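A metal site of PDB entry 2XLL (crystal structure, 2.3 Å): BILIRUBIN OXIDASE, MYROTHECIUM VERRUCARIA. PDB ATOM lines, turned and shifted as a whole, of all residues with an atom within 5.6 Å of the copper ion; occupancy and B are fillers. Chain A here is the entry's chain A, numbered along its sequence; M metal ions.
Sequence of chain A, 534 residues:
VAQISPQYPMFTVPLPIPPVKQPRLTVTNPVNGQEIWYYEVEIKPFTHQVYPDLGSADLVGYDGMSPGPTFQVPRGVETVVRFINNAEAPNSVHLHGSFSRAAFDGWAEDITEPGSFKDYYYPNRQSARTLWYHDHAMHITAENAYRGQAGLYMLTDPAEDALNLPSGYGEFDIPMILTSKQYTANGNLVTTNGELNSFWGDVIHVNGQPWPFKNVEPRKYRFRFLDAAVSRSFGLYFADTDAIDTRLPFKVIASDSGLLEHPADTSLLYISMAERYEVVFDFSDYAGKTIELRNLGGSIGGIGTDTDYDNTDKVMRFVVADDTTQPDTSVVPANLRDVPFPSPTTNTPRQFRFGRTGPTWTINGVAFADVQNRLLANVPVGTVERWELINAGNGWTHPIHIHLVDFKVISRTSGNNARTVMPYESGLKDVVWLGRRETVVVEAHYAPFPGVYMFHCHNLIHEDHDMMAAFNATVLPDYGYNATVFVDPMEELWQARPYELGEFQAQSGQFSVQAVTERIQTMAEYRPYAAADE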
ATOM      1  N   TRP A 361      19.231  19.163  20.144  1.00  0.00           N
ATOM      2  CA  TRP A 361      20.084  18.766  21.252  1.00  0.00           C
ATOM      3  C   TRP A 361      21.517  19.004  20.849  1.00  0.00           C
ATOM      4  O   TRP A 361      21.952  18.538  19.809  1.00  0.00           O
ATOM      5  CB  TRP A 361      19.891  17.285  21.596  1.00  0.00           C
ATOM      6  CG  TRP A 361      18.494  16.922  22.028  1.00  0.00           C
ATOM      7  CD1 TRP A 361      17.564  16.233  21.293  1.00  0.00           C
ATOM      8  CD2 TRP A 361      17.874  17.197  23.295  1.00  0.00           C
ATOM      9  NE1 TRP A 361      16.409  16.075  22.022  1.00  0.00           N
ATOM     10  CE2 TRP A 361      16.579  16.658  23.259  1.00  0.00           C
ATOM     11  CE3 TRP A 361      18.302  17.864  24.443  1.00  0.00           C
ATOM     12  CZ2 TRP A 361      15.696  16.760  24.325  1.00  0.00           C
ATOM     13  CZ3 TRP A 361      17.424  17.958  25.510  1.00  0.00           C
ATOM     14  CH2 TRP A 361      16.133  17.406  25.447  1.00  0.00           C
ATOM     15  N   THR A 397      18.134  14.429  31.058  1.00  0.00           N
ATOM     16  CA  THR A 397      19.361  13.868  31.611  1.00  0.00           C
ATOM     17  C   THR A 397      20.160  13.269  30.484  1.00  0.00           C
ATOM     18  O   THR A 397      19.597  12.983  29.415  1.00  0.00           O
ATOM     19  CB  THR A 397      19.112  12.795  32.684  1.00  0.00           C
ATOM     20  OG1 THR A 397      18.542  11.619  32.087  1.00  0.00           O
ATOM     21  CG2 THR A 397      18.176  13.337  33.753  1.00  0.00           C
ATOM     22  N   HIS A 398      21.466  13.092  30.698  1.00  0.00           N
ATOM     23  CA  HIS A 398      22.356  12.684  29.621  1.00  0.00           C
ATOM     24  C   HIS A 398      23.497  11.805  30.077  1.00  0.00           C
ATOM     25  O   HIS A 398      24.385  12.263  30.787  1.00  0.00           O
ATOM     26  CB  HIS A 398      22.914  13.917  28.948  1.00  0.00           C
ATOM     27  CG  HIS A 398      21.863  14.916  28.636  1.00  0.00           C
ATOM     28  ND1 HIS A 398      21.023  14.787  27.546  1.00  0.00           N
ATOM     29  CD2 HIS A 398      21.454  16.030  29.297  1.00  0.00           C
ATOM     30  CE1 HIS A 398      20.169  15.797  27.529  1.00  0.00           C
ATOM     31  NE2 HIS A 398      20.409  16.557  28.575  1.00  0.00           N
ATOM     32  N   PRO A 399      23.456  10.523  29.681  1.00  0.00           N
ATOM     33  CA  PRO A 399      24.569   9.617  29.914  1.00  0.00           C
ATOM     34  C   PRO A 399      25.638   9.912  28.865  1.00  0.00           C
ATOM     35  O   PRO A 399      25.425   9.610  27.694  1.00  0.00           O
ATOM     36  CB  PRO A 399      23.942   8.222  29.698  1.00  0.00           C
ATOM     37  CG  PRO A 399      22.817   8.464  28.724  1.00  0.00           C
ATOM     38  CD  PRO A 399      22.322   9.876  28.973  1.00  0.00           C
ATOM     39  N   CYS A 457      26.064  12.194  23.993  1.00  0.00           N
ATOM     40  CA  CYS A 457      25.106  11.590  24.891  1.00  0.00           C
ATOM     41  C   CYS A 457      24.695  10.238  24.308  1.00  0.00           C
ATOM     42  O   CYS A 457      24.565  10.091  23.106  1.00  0.00           O
ATOM     43  CB  CYS A 457      23.876  12.482  25.030  1.00  0.00           C
ATOM     44  SG  CYS A 457      22.604  11.749  26.089  1.00  0.00           S
ATOM     45  N   HIS A 458      24.443   9.257  25.162  1.00  0.00           N
ATOM     46  CA  HIS A 458      24.052   7.956  24.637  1.00  0.00           C
ATOM     47  C   HIS A 458      22.531   7.714  24.688  1.00  0.00           C
ATOM     48  O   HIS A 458      22.050   6.599  24.435  1.00  0.00           O
ATOM     49  CB  HIS A 458      24.824   6.823  25.330  1.00  0.00           C
ATOM     50  CG  HIS A 458      25.214   5.717  24.397  1.00  0.00           C
ATOM     51  ND1 HIS A 458      24.298   4.811  23.904  1.00  0.00           N
ATOM     52  CD2 HIS A 458      26.405   5.390  23.858  1.00  0.00           C
ATOM     53  CE1 HIS A 458      24.917   3.956  23.105  1.00  0.00           C
ATOM     54  NE2 HIS A 458      26.193   4.283  23.062  1.00  0.00           N
ATOM     55  N   ASN A 459      21.780   8.757  25.005  1.00  0.00           N
ATOM     56  CA  ASN A 459      20.353   8.747  24.707  1.00  0.00           C
ATOM     57  C   ASN A 459      20.296   8.835  23.192  1.00  0.00           C
ATOM     58  O   ASN A 459      20.595   9.883  22.627  1.00  0.00           O
ATOM     59  CB  ASN A 459      19.664   9.947  25.350  1.00  0.00           C
ATOM     60  CG  ASN A 459      18.184   9.977  25.050  1.00  0.00           C
ATOM     61  OD1 ASN A 459      17.764   9.772  23.920  1.00  0.00           O
ATOM     62  ND2 ASN A 459      17.367  10.237  26.085  1.00  0.00           N
ATOM     63  N   HIS A 462      18.571  11.786  21.555  1.00  0.00           N
ATOM     64  CA  HIS A 462      19.370  13.013  21.669  1.00  0.00           C
ATOM     65  C   HIS A 462      20.559  12.950  20.718  1.00  0.00           C
ATOM     66  O   HIS A 462      20.858  13.903  20.008  1.00  0.00           O
ATOM     67  CB  HIS A 462      19.866  13.187  23.107  1.00  0.00           C
ATOM     68  CG  HIS A 462      18.767  13.348  24.091  1.00  0.00           C
ATOM     69  ND1 HIS A 462      18.961  13.329  25.447  1.00  0.00           N
ATOM     70  CD2 HIS A 462      17.432  13.524  23.907  1.00  0.00           C
ATOM     71  CE1 HIS A 462      17.805  13.501  26.069  1.00  0.00           C
ATOM     72  NE2 HIS A 462      16.857  13.617  25.152  1.00  0.00           N
ATOM     73  N   MET A 467      23.076  15.550  19.454  1.00  0.00           N
ATOM     74  CA  MET A 467      23.972  15.792  20.570  1.00  0.00           C
ATOM     75  C   MET A 467      25.256  14.944  20.472  1.00  0.00           C
ATOM     76  O   MET A 467      25.517  14.098  21.304  1.00  0.00           O
ATOM     77  CB  MET A 467      23.235  15.519  21.877  1.00  0.00           C
ATOM     78  CG  MET A 467      23.962  15.991  23.129  1.00  0.00           C
ATOM     79  SD  MET A 467      22.933  15.770  24.580  1.00  0.00           S
ATOM     80  CE  MET A 467      22.300  17.432  24.761  1.00  0.00           C
HETATM   81 CU    CU M   1      20.999  13.411  26.140  1.00  0.00          CU
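N of Cys 457 lies within hydrogen-bond range of O of Met 467, at 3.3 Å. The backbone NH (N) of His 462 is in hydrogen-bond range of the side-chain amide oxygen (OD1) of Asn 459, 3.2 Å away. The backbone NH (N) of Met 467 lies within hydrogen-bond range of the backbone carbonyl oxygen (O) of Trp 361, at 3.2 Å. The side-chain sulfur (SG) of Cys 457 lies close to the backbone NH (N) of Asn 459 (3.3 Å). O of His 462 is in hydrogen-bond range of N of Met 467 (2.8 Å). ND1 of His 398 lies close to SD of Met 467, 3.7 Å away.
O of Thr 397 touches the copper ion, at 3.6 Å. Asn 459 touches the copper ion. Met 467 touches the copper ion. Six residues have an atom within 4 Å of the copper ion: Thr 397, His 398, Cys 457, Asn 459, His 462 and Met 467.
The copper ion is bound by ND1 of His 398 (2.0 Å). A ring nitrogen (ND1) of His 462 binds the copper ion, at 2.2 Å. The side-chain sulfur (SG) of Cys 457 is bound to the copper ion (2.3 Å). The copper ion has three donor atoms within binding distance.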
